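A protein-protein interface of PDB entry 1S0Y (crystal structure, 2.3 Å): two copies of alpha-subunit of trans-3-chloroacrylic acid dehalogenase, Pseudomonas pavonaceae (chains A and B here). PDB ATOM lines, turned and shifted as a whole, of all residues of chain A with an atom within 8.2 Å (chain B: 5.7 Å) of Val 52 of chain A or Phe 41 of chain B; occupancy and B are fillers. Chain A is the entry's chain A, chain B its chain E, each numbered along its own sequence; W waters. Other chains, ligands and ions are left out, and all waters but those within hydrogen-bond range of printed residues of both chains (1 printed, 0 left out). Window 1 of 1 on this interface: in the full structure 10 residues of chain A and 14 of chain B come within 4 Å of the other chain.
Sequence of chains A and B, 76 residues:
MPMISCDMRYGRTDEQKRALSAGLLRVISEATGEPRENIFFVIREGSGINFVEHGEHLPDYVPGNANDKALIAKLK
Water W1 lies within hydrogen-bond range of the side-chain hydroxyl (OG) of Ser 21 of chain B (2.6 Å) and the backbone carbonyl oxygen (O) of Gly 55 of chain A (3.0 Å).
No position is printed for both chains. Of the 14 pairs that touch across the chains among the printed residues, none has its exchanged pair printed and touching as well.
Printed residues of chain B within 4 Å of Val 52 of chain A: Ser 21, Phe 40 and Phe 41. Of chain A, only Asn 50, Phe 51 and Val 52 come within 4 Å of Phe 41 of chain B. Of the printed residues of chain A, Ile 39 of chain B touches His 54. Of the printed residues of chain A, Ser 21 of chain B touches Val 52 (3.98 Å) and His 57 (2.7 Å). Cys 6 of chain B touches none of the printed residues of chain A. Leu 24 of chain B touches none of the printed residues of chain A. The nearest printed residue of chain B that does not touch Val 52 of chain A is Ile 39 of chain B (4.3 Å). The nearest printed residue of chain A that does not touch Lys 17 of chain B is Ser 47 of chain A (5.4 Å).
A ring nitrogen (NE2) of His 57 of chain A is in hydrogen-bond range of the side-chain hydroxyl (OG) of Ser 21 of chain B (2.7 Å). The side-chain amide oxygen of Asn 50 of chain A sits at hydrogen-bond distance from the side-chain amino group of Lys 17 of chain B (2.7 Å). The backbone NH of Val 52 of chain A lies within hydrogen-bond range of the backbone carbonyl oxygen of Phe 41 of chain B (2.8 Å). The backbone carbonyl oxygen (O) of Asn 50 of chain A is in hydrogen-bond range of the backbone NH (N) of Ile 43 of chain B (2.9 Å).
Of the 14 printed residues of chain A, 8 touch a printed residue of chain B. Printed residues of chain A that touch a printed residue of chain B: Ile 49, Asn 50, Phe 51, Val 52, Glu 53, His 54, Gly 55 and His 57. Hydrophobic or aromatic side chains of chain A that line the printed part of chain B: Ile 49, Val 52 and His 57. Hydrophobic or aromatic side chains of chain B that line the printed part of chain A: Leu 25, Phe 40, Phe 41, Val 42 and Ile 43. Among the printed residues, no Asp or Glu carboxylate lies within 4 Å of a Lys or Arg side-chain nitrogen of the other chain.
O of Val 42 of chain B lies within hydrogen-bond range of N of Cys 6 of chain B (2.8 Å). The backbone NH of Ile 4 of chain B is in hydrogen-bond range of the backbone carbonyl oxygen of Phe 40 of chain B, at 2.8 Å. N of Val 42 of chain B lies within hydrogen-bond range of O of Ile 4 of chain B (2.9 Å). The backbone NH (N) of Leu 58 of chain A is in hydrogen-bond range of the backbone carbonyl oxygen (O) of Phe 51 of chain A (2.7 Å). The backbone carbonyl oxygen of Ile 49 of chain A sits at hydrogen-bond distance from a ring nitrogen (ND1) of His 57 of chain A (2.7 Å). The backbone carbonyl oxygen of Leu 58 of chain A sits at hydrogen-bond distance from the backbone NH of Ile 49 of chain A.
Ile 49 of chain A touches Lys 17 of chain B. Phe 41 of chain B touches Asn 50 of chain A (O to O, 3.8 Å). Asn 50 of chain A touches Val 42 of chain B. Phe 41 of chain B touches Phe 51 of chain A (O to C, 3.8 Å). Val 52 of chain A touches Ser 21 of chain B. Val 52 of chain A touches Phe 40 of chain B (O to CD1, 3.3 Å). Glu 53 of chain A touches Phe 40 of chain B (OE2 to CE1, 3.4 Å). O of Ile 39 of chain B touches N of His 54 of chain A (3.9 Å). Gly 55 of chain A touches Leu 25 of chain B (CA to CD2, 3.7 Å). His 57 of chain A touches Lys 17 of chain B (CE1 to O, 3.5 Å).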
ATOM      1  N   ARG A   9      12.873   7.673  25.233  1.00  0.00           N
ATOM      2  CA  ARG A   9      12.723   8.986  24.611  1.00  0.00           C
ATOM      3  C   ARG A   9      13.276  10.111  25.498  1.00  0.00           C
ATOM      4  O   ARG A   9      13.269   9.992  26.726  1.00  0.00           O
ATOM      5  CB  ARG A   9      11.243   9.266  24.329  1.00  0.00           C
ATOM      6  CG  ARG A   9      10.549   8.265  23.412  1.00  0.00           C
ATOM      7  CD  ARG A   9       9.059   8.610  23.240  1.00  0.00           C
ATOM      8  NE  ARG A   9       8.268   8.283  24.430  1.00  0.00           N
ATOM      9  CZ  ARG A   9       7.035   8.735  24.679  1.00  0.00           C
ATOM     10  NH1 ARG A   9       6.415   9.547  23.828  1.00  0.00           N
ATOM     11  NH2 ARG A   9       6.414   8.372  25.791  1.00  0.00           N
ATOM     12  N   SER A  47      14.586  10.809  19.899  1.00  0.00           N
ATOM     13  CA  SER A  47      13.307  11.472  19.627  1.00  0.00           C
ATOM     14  C   SER A  47      12.222  10.397  19.584  1.00  0.00           C
ATOM     15  O   SER A  47      12.514   9.238  19.307  1.00  0.00           O
ATOM     16  CB  SER A  47      13.346  12.174  18.271  1.00  0.00           C
ATOM     17  OG  SER A  47      14.382  13.135  18.226  1.00  0.00           O
ATOM     18  N   GLY A  48      10.976  10.787  19.851  1.00  0.00           N
ATOM     19  CA  GLY A  48       9.881   9.836  19.827  1.00  0.00           C
ATOM     20  C   GLY A  48       9.778   9.132  18.484  1.00  0.00           C
ATOM     21  O   GLY A  48       9.478   7.934  18.429  1.00  0.00           O
ATOM     22  N   ILE A  49      10.022   9.859  17.396  1.00  0.00           N
ATOM     23  CA  ILE A  49       9.947   9.258  16.069  1.00  0.00           C
ATOM     24  C   ILE A  49      10.898   8.056  16.007  1.00  0.00           C
ATOM     25  O   ILE A  49      10.674   7.110  15.233  1.00  0.00           O
ATOM     26  CB  ILE A  49      10.305  10.299  14.954  1.00  0.00           C
ATOM     27  CG1 ILE A  49      10.297   9.642  13.564  1.00  0.00           C
ATOM     28  CG2 ILE A  49      11.651  10.915  15.228  1.00  0.00           C
ATOM     29  CD1 ILE A  49       8.928   9.491  12.944  1.00  0.00           C
ATOM     30  N   ASN A  50      11.941   8.079  16.842  1.00  0.00           N
ATOM     31  CA  ASN A  50      12.919   6.983  16.889  1.00  0.00           C
ATOM     32  C   ASN A  50      12.438   5.781  17.685  1.00  0.00           C
ATOM     33  O   ASN A  50      13.117   4.751  17.723  1.00  0.00           O
ATOM     34  CB  ASN A  50      14.248   7.435  17.506  1.00  0.00           C
ATOM     35  CG  ASN A  50      15.044   8.332  16.593  1.00  0.00           C
ATOM     36  OD1 ASN A  50      14.688   8.533  15.427  1.00  0.00           O
ATOM     37  ND2 ASN A  50      16.139   8.875  17.113  1.00  0.00           N
ATOM     38  N   PHE A  51      11.291   5.914  18.339  1.00  0.00           N
ATOM     39  CA  PHE A  51      10.752   4.817  19.133  1.00  0.00           C
ATOM     40  C   PHE A  51       9.473   4.270  18.532  1.00  0.00           C
ATOM     41  O   PHE A  51       8.432   4.926  18.555  1.00  0.00           O
ATOM     42  CB  PHE A  51      10.500   5.272  20.565  1.00  0.00           C
ATOM     43  CG  PHE A  51      11.737   5.338  21.391  1.00  0.00           C
ATOM     44  CD1 PHE A  51      12.700   6.307  21.142  1.00  0.00           C
ATOM     45  CD2 PHE A  51      11.974   4.391  22.390  1.00  0.00           C
ATOM     46  CE1 PHE A  51      13.887   6.331  21.873  1.00  0.00           C
ATOM     47  CE2 PHE A  51      13.151   4.406  23.125  1.00  0.00           C
ATOM     48  CZ  PHE A  51      14.114   5.377  22.865  1.00  0.00           C
ATOM     49  N   VAL A  52       9.554   3.057  18.000  1.00  0.00           N
ATOM     50  CA  VAL A  52       8.400   2.436  17.375  1.00  0.00           C
ATOM     51  C   VAL A  52       7.810   1.344  18.256  1.00  0.00           C
ATOM     52  O   VAL A  52       8.429   0.300  18.467  1.00  0.00           O
ATOM     53  CB  VAL A  52       8.794   1.837  16.015  1.00  0.00           C
ATOM     54  CG1 VAL A  52       7.555   1.385  15.266  1.00  0.00           C
ATOM     55  CG2 VAL A  52       9.577   2.866  15.212  1.00  0.00           C
ATOM     56  N   GLU A  53       6.616   1.593  18.779  1.00  0.00           N
ATOM     57  CA  GLU A  53       5.930   0.623  19.627  1.00  0.00           C
ATOM     58  C   GLU A  53       4.771   0.006  18.853  1.00  0.00           C
ATOM     59  O   GLU A  53       3.993   0.713  18.215  1.00  0.00           O
ATOM     60  CB  GLU A  53       5.375   1.296  20.881  1.00  0.00           C
ATOM     61  CG  GLU A  53       6.404   2.043  21.693  1.00  0.00           C
ATOM     62  CD  GLU A  53       7.219   1.133  22.577  1.00  0.00           C
ATOM     63  OE1 GLU A  53       6.957  -0.088  22.590  1.00  0.00           O
ATOM     64  OE2 GLU A  53       8.122   1.645  23.267  1.00  0.00           O
ATOM     65  N   HIS A  54       4.667  -1.315  18.901  1.00  0.00           N
ATOM     66  CA  HIS A  54       3.590  -2.010  18.216  1.00  0.00           C
ATOM     67  C   HIS A  54       3.485  -1.607  16.749  1.00  0.00           C
ATOM     68  O   HIS A  54       2.457  -1.837  16.117  1.00  0.00           O
ATOM     69  CB  HIS A  54       2.261  -1.719  18.925  1.00  0.00           C
ATOM     70  CG  HIS A  54       2.315  -1.930  20.406  1.00  0.00           C
ATOM     71  ND1 HIS A  54       2.092  -0.913  21.311  1.00  0.00           N
ATOM     72  CD2 HIS A  54       2.590  -3.035  21.141  1.00  0.00           C
ATOM     73  CE1 HIS A  54       2.230  -1.383  22.539  1.00  0.00           C
ATOM     74  NE2 HIS A  54       2.532  -2.666  22.463  1.00  0.00           N
ATOM     75  N   GLY A  55       4.541  -1.008  16.206  1.00  0.00           N
ATOM     76  CA  GLY A  55       4.507  -0.597  14.811  1.00  0.00           C
ATOM     77  C   GLY A  55       4.286   0.892  14.579  1.00  0.00           C
ATOM     78  O   GLY A  55       4.526   1.399  13.484  1.00  0.00           O
ATOM     79  N   GLU A  56       3.826   1.602  15.599  1.00  0.00           N
ATOM     80  CA  GLU A  56       3.601   3.032  15.461  1.00  0.00           C
ATOM     81  C   GLU A  56       4.715   3.819  16.159  1.00  0.00           C
ATOM     82  O   GLU A  56       5.097   3.505  17.285  1.00  0.00           O
ATOM     83  CB  GLU A  56       2.233   3.405  16.049  1.00  0.00           C
ATOM     84  N   HIS A  57       5.242   4.836  15.486  1.00  0.00           N
ATOM     85  CA  HIS A  57       6.290   5.655  16.076  1.00  0.00           C
ATOM     86  C   HIS A  57       5.678   6.547  17.148  1.00  0.00           C
ATOM     87  O   HIS A  57       4.627   7.157  16.934  1.00  0.00           O
ATOM     88  CB  HIS A  57       6.973   6.511  15.009  1.00  0.00           C
ATOM     89  CG  HIS A  57       7.640   5.712  13.935  1.00  0.00           C
ATOM     90  ND1 HIS A  57       8.958   5.901  13.576  1.00  0.00           N
ATOM     91  CD2 HIS A  57       7.167   4.730  13.131  1.00  0.00           C
ATOM     92  CE1 HIS A  57       9.267   5.072  12.595  1.00  0.00           C
ATOM     93  NE2 HIS A  57       8.197   4.351  12.306  1.00  0.00           N
ATOM     94  N   LEU A  58       6.335   6.610  18.302  1.00  0.00           N
ATOM     95  CA  LEU A  58       5.859   7.417  19.412  1.00  0.00           C
ATOM     96  C   LEU A  58       6.098   8.897  19.175  1.00  0.00           C
ATOM     97  O   LEU A  58       7.028   9.283  18.469  1.00  0.00           O
ATOM     98  CB  LEU A  58       6.560   7.015  20.715  1.00  0.00           C
ATOM     99  CG  LEU A  58       6.503   5.552  21.154  1.00  0.00           C
ATOM    100  CD1 LEU A  58       7.177   5.407  22.514  1.00  0.00           C
ATOM    101  CD2 LEU A  58       5.058   5.092  21.233  1.00  0.00           C
ATOM    102  N   PRO A  59       5.238   9.749  19.745  1.00  0.00           N
ATOM    103  CA  PRO A  59       5.401  11.196  19.580  1.00  0.00           C
ATOM    104  C   PRO A  59       6.475  11.592  20.580  1.00  0.00           C
ATOM    105  O   PRO A  59       6.771  10.822  21.499  1.00  0.00           O
ATOM    106  CB  PRO A  59       4.036  11.739  19.973  1.00  0.00           C
ATOM    107  CG  PRO A  59       3.626  10.794  21.086  1.00  0.00           C
ATOM    108  CD  PRO A  59       4.022   9.434  20.520  1.00  0.00           C
ATOM    109  N   MET B   3      12.902  -7.605  19.479  1.00  0.00           N
ATOM    110  CA  MET B   3      13.338  -6.214  19.578  1.00  0.00           C
ATOM    111  C   MET B   3      14.473  -5.904  18.597  1.00  0.00           C
ATOM    112  O   MET B   3      15.475  -6.617  18.537  1.00  0.00           O
ATOM    113  CB  MET B   3      13.804  -5.876  20.996  1.00  0.00           C
ATOM    114  CG  MET B   3      12.733  -6.014  22.055  1.00  0.00           C
ATOM    115  SD  MET B   3      12.691  -7.672  22.751  1.00  0.00           S
ATOM    116  CE  MET B   3      12.728  -7.276  24.507  1.00  0.00           C
ATOM    117  N   ILE B   4      14.302  -4.836  17.828  1.00  0.00           N
ATOM    118  CA  ILE B   4      15.306  -4.423  16.863  1.00  0.00           C
ATOM    119  C   ILE B   4      15.820  -3.015  17.167  1.00  0.00           C
ATOM    120  O   ILE B   4      15.048  -2.123  17.503  1.00  0.00           O
ATOM    121  CB  ILE B   4      14.749  -4.404  15.423  1.00  0.00           C
ATOM    122  CG1 ILE B   4      14.250  -5.785  15.020  1.00  0.00           C
ATOM    123  CG2 ILE B   4      15.832  -3.955  14.464  1.00  0.00           C
ATOM    124  CD1 ILE B   4      12.843  -6.068  15.456  1.00  0.00           C
ATOM    125  N   SER B   5      17.129  -2.825  17.053  1.00  0.00           N
ATOM    126  CA  SER B   5      17.713  -1.514  17.271  1.00  0.00           C
ATOM    127  C   SER B   5      18.531  -1.180  16.031  1.00  0.00           C
ATOM    128  O   SER B   5      19.147  -2.061  15.421  1.00  0.00           O
ATOM    129  CB  SER B   5      18.625  -1.504  18.501  1.00  0.00           C
ATOM    130  OG  SER B   5      19.793  -2.270  18.269  1.00  0.00           O
ATOM    131  N   CYS B   6      18.523   0.092  15.652  1.00  0.00           N
ATOM    132  CA  CYS B   6      19.277   0.541  14.497  1.00  0.00           C
ATOM    133  C   CYS B   6      20.107   1.768  14.825  1.00  0.00           C
ATOM    134  O   CYS B   6      19.560   2.828  15.123  1.00  0.00           O
ATOM    135  CB  CYS B   6      18.337   0.863  13.332  1.00  0.00           C
ATOM    136  SG  CYS B   6      19.175   1.682  11.930  1.00  0.00           S
ATOM    137  N   LYS B  17      12.587   7.072   8.103  1.00  0.00           N
ATOM    138  CA  LYS B  17      12.469   6.299   9.335  1.00  0.00           C
ATOM    139  C   LYS B  17      11.205   5.446   9.334  1.00  0.00           C
ATOM    140  O   LYS B  17      11.231   4.289   9.751  1.00  0.00           O
ATOM    141  CB  LYS B  17      12.468   7.227  10.552  1.00  0.00           C
ATOM    142  CG  LYS B  17      13.795   7.947  10.773  1.00  0.00           C
ATOM    143  CD  LYS B  17      13.764   8.820  12.007  1.00  0.00           C
ATOM    144  CE  LYS B  17      15.104   9.510  12.247  1.00  0.00           C
ATOM    145  NZ  LYS B  17      15.098  10.326  13.500  1.00  0.00           N
ATOM    146  N   LEU B  20      11.570   2.575   7.085  1.00  0.00           N
ATOM    147  CA  LEU B  20      12.575   1.686   7.648  1.00  0.00           C
ATOM    148  C   LEU B  20      11.919   0.711   8.619  1.00  0.00           C
ATOM    149  O   LEU B  20      12.121  -0.500   8.518  1.00  0.00           O
ATOM    150  CB  LEU B  20      13.650   2.487   8.385  1.00  0.00           C
ATOM    151  CG  LEU B  20      15.069   1.905   8.463  1.00  0.00           C
ATOM    152  CD1 LEU B  20      15.716   2.343   9.772  1.00  0.00           C
ATOM    153  CD2 LEU B  20      15.047   0.396   8.364  1.00  0.00           C
ATOM    154  N   SER B  21      11.135   1.234   9.559  1.00  0.00           N
ATOM    155  CA  SER B  21      10.472   0.368  10.531  1.00  0.00           C
ATOM    156  C   SER B  21       9.481  -0.565   9.835  1.00  0.00           C
ATOM    157  O   SER B  21       9.371  -1.743  10.189  1.00  0.00           O
ATOM    158  CB  SER B  21       9.755   1.200  11.601  1.00  0.00           C
ATOM    159  OG  SER B  21       8.690   1.954  11.055  1.00  0.00           O
ATOM    160  N   LEU B  24      11.511  -3.301   8.142  1.00  0.00           N
ATOM    161  CA  LEU B  24      12.066  -4.136   9.205  1.00  0.00           C
ATOM    162  C   LEU B  24      11.027  -4.990   9.928  1.00  0.00           C
ATOM    163  O   LEU B  24      11.274  -6.160  10.226  1.00  0.00           O
ATOM    164  CB  LEU B  24      12.804  -3.262  10.220  1.00  0.00           C
ATOM    165  CG  LEU B  24      14.327  -3.148  10.109  1.00  0.00           C
ATOM    166  CD1 LEU B  24      14.790  -3.267   8.682  1.00  0.00           C
ATOM    167  CD2 LEU B  24      14.763  -1.841  10.712  1.00  0.00           C
ATOM    168  N   LEU B  25       9.864  -4.422  10.215  1.00  0.00           N
ATOM    169  CA  LEU B  25       8.849  -5.198  10.907  1.00  0.00           C
ATOM    170  C   LEU B  25       8.238  -6.275  10.027  1.00  0.00           C
ATOM    171  O   LEU B  25       7.717  -7.272  10.524  1.00  0.00           O
ATOM    172  CB  LEU B  25       7.755  -4.280  11.470  1.00  0.00           C
ATOM    173  CG  LEU B  25       7.965  -3.944  12.953  1.00  0.00           C
ATOM    174  CD1 LEU B  25       9.371  -3.397  13.167  1.00  0.00           C
ATOM    175  CD2 LEU B  25       6.920  -2.961  13.421  1.00  0.00           C
ATOM    176  N   ILE B  39       6.549  -6.653  18.057  1.00  0.00           N
ATOM    177  CA  ILE B  39       7.857  -6.170  17.620  1.00  0.00           C
ATOM    178  C   ILE B  39       8.178  -4.740  18.082  1.00  0.00           C
ATOM    179  O   ILE B  39       7.428  -3.801  17.814  1.00  0.00           O
ATOM    180  CB  ILE B  39       7.966  -6.230  16.068  1.00  0.00           C
ATOM    181  CG1 ILE B  39       7.746  -7.664  15.582  1.00  0.00           C
ATOM    182  CG2 ILE B  39       9.333  -5.730  15.607  1.00  0.00           C
ATOM    183  CD1 ILE B  39       7.570  -7.778  14.070  1.00  0.00           C
ATOM    184  N   PHE B  40       9.289  -4.573  18.790  1.00  0.00           N
ATOM    185  CA  PHE B  40       9.693  -3.240  19.228  1.00  0.00           C
ATOM    186  C   PHE B  40      10.907  -2.803  18.426  1.00  0.00           C
ATOM    187  O   PHE B  40      11.840  -3.589  18.224  1.00  0.00           O
ATOM    188  CB  PHE B  40      10.074  -3.208  20.702  1.00  0.00           C
ATOM    189  CG  PHE B  40      10.774  -1.937  21.102  1.00  0.00           C
ATOM    190  CD1 PHE B  40      10.071  -0.734  21.181  1.00  0.00           C
ATOM    191  CD2 PHE B  40      12.144  -1.929  21.349  1.00  0.00           C
ATOM    192  CE1 PHE B  40      10.725   0.452  21.503  1.00  0.00           C
ATOM    193  CE2 PHE B  40      12.805  -0.748  21.670  1.00  0.00           C
ATOM    194  CZ  PHE B  40      12.097   0.443  21.748  1.00  0.00           C
ATOM    195  N   PHE B  41      10.905  -1.552  17.980  1.00  0.00           N
ATOM    196  CA  PHE B  41      12.031  -1.038  17.209  1.00  0.00           C
ATOM    197  C   PHE B  41      12.490   0.340  17.694  1.00  0.00           C
ATOM    198  O   PHE B  41      11.674   1.233  17.957  1.00  0.00           O
ATOM    199  CB  PHE B  41      11.656  -0.992  15.724  1.00  0.00           C
ATOM    200  CG  PHE B  41      12.706  -0.366  14.838  1.00  0.00           C
ATOM    201  CD1 PHE B  41      14.041  -0.780  14.904  1.00  0.00           C
ATOM    202  CD2 PHE B  41      12.345   0.597  13.890  1.00  0.00           C
ATOM    203  CE1 PHE B  41      15.003  -0.250  14.033  1.00  0.00           C
ATOM    204  CE2 PHE B  41      13.296   1.138  13.007  1.00  0.00           C
ATOM    205  CZ  PHE B  41      14.630   0.714  13.078  1.00  0.00           C
ATOM    206  N   VAL B  42      13.805   0.485  17.827  1.00  0.00           N
ATOM    207  CA  VAL B  42      14.425   1.731  18.262  1.00  0.00           C
ATOM    208  C   VAL B  42      15.582   2.148  17.352  1.00  0.00           C
ATOM    209  O   VAL B  42      16.410   1.326  16.936  1.00  0.00           O
ATOM    210  CB  VAL B  42      14.998   1.623  19.670  1.00  0.00           C
ATOM    211  CG1 VAL B  42      16.024   0.497  19.723  1.00  0.00           C
ATOM    212  CG2 VAL B  42      15.655   2.949  20.059  1.00  0.00           C
ATOM    213  N   ILE B  43      15.644   3.444  17.087  1.00  0.00           N
ATOM    214  CA  ILE B  43      16.673   4.034  16.253  1.00  0.00           C
ATOM    215  C   ILE B  43      17.582   4.863  17.158  1.00  0.00           C
ATOM    216  O   ILE B  43      17.095   5.548  18.044  1.00  0.00           O
ATOM    217  CB  ILE B  43      16.009   4.946  15.184  1.00  0.00           C
ATOM    218  CG1 ILE B  43      15.157   4.084  14.238  1.00  0.00           C
ATOM    219  CG2 ILE B  43      17.052   5.741  14.436  1.00  0.00           C
ATOM    220  CD1 ILE B  43      14.322   4.886  13.222  1.00  0.00           C
HETATM  221  O   HOH W   1       6.199   1.065  11.067  1.00  0.00           O
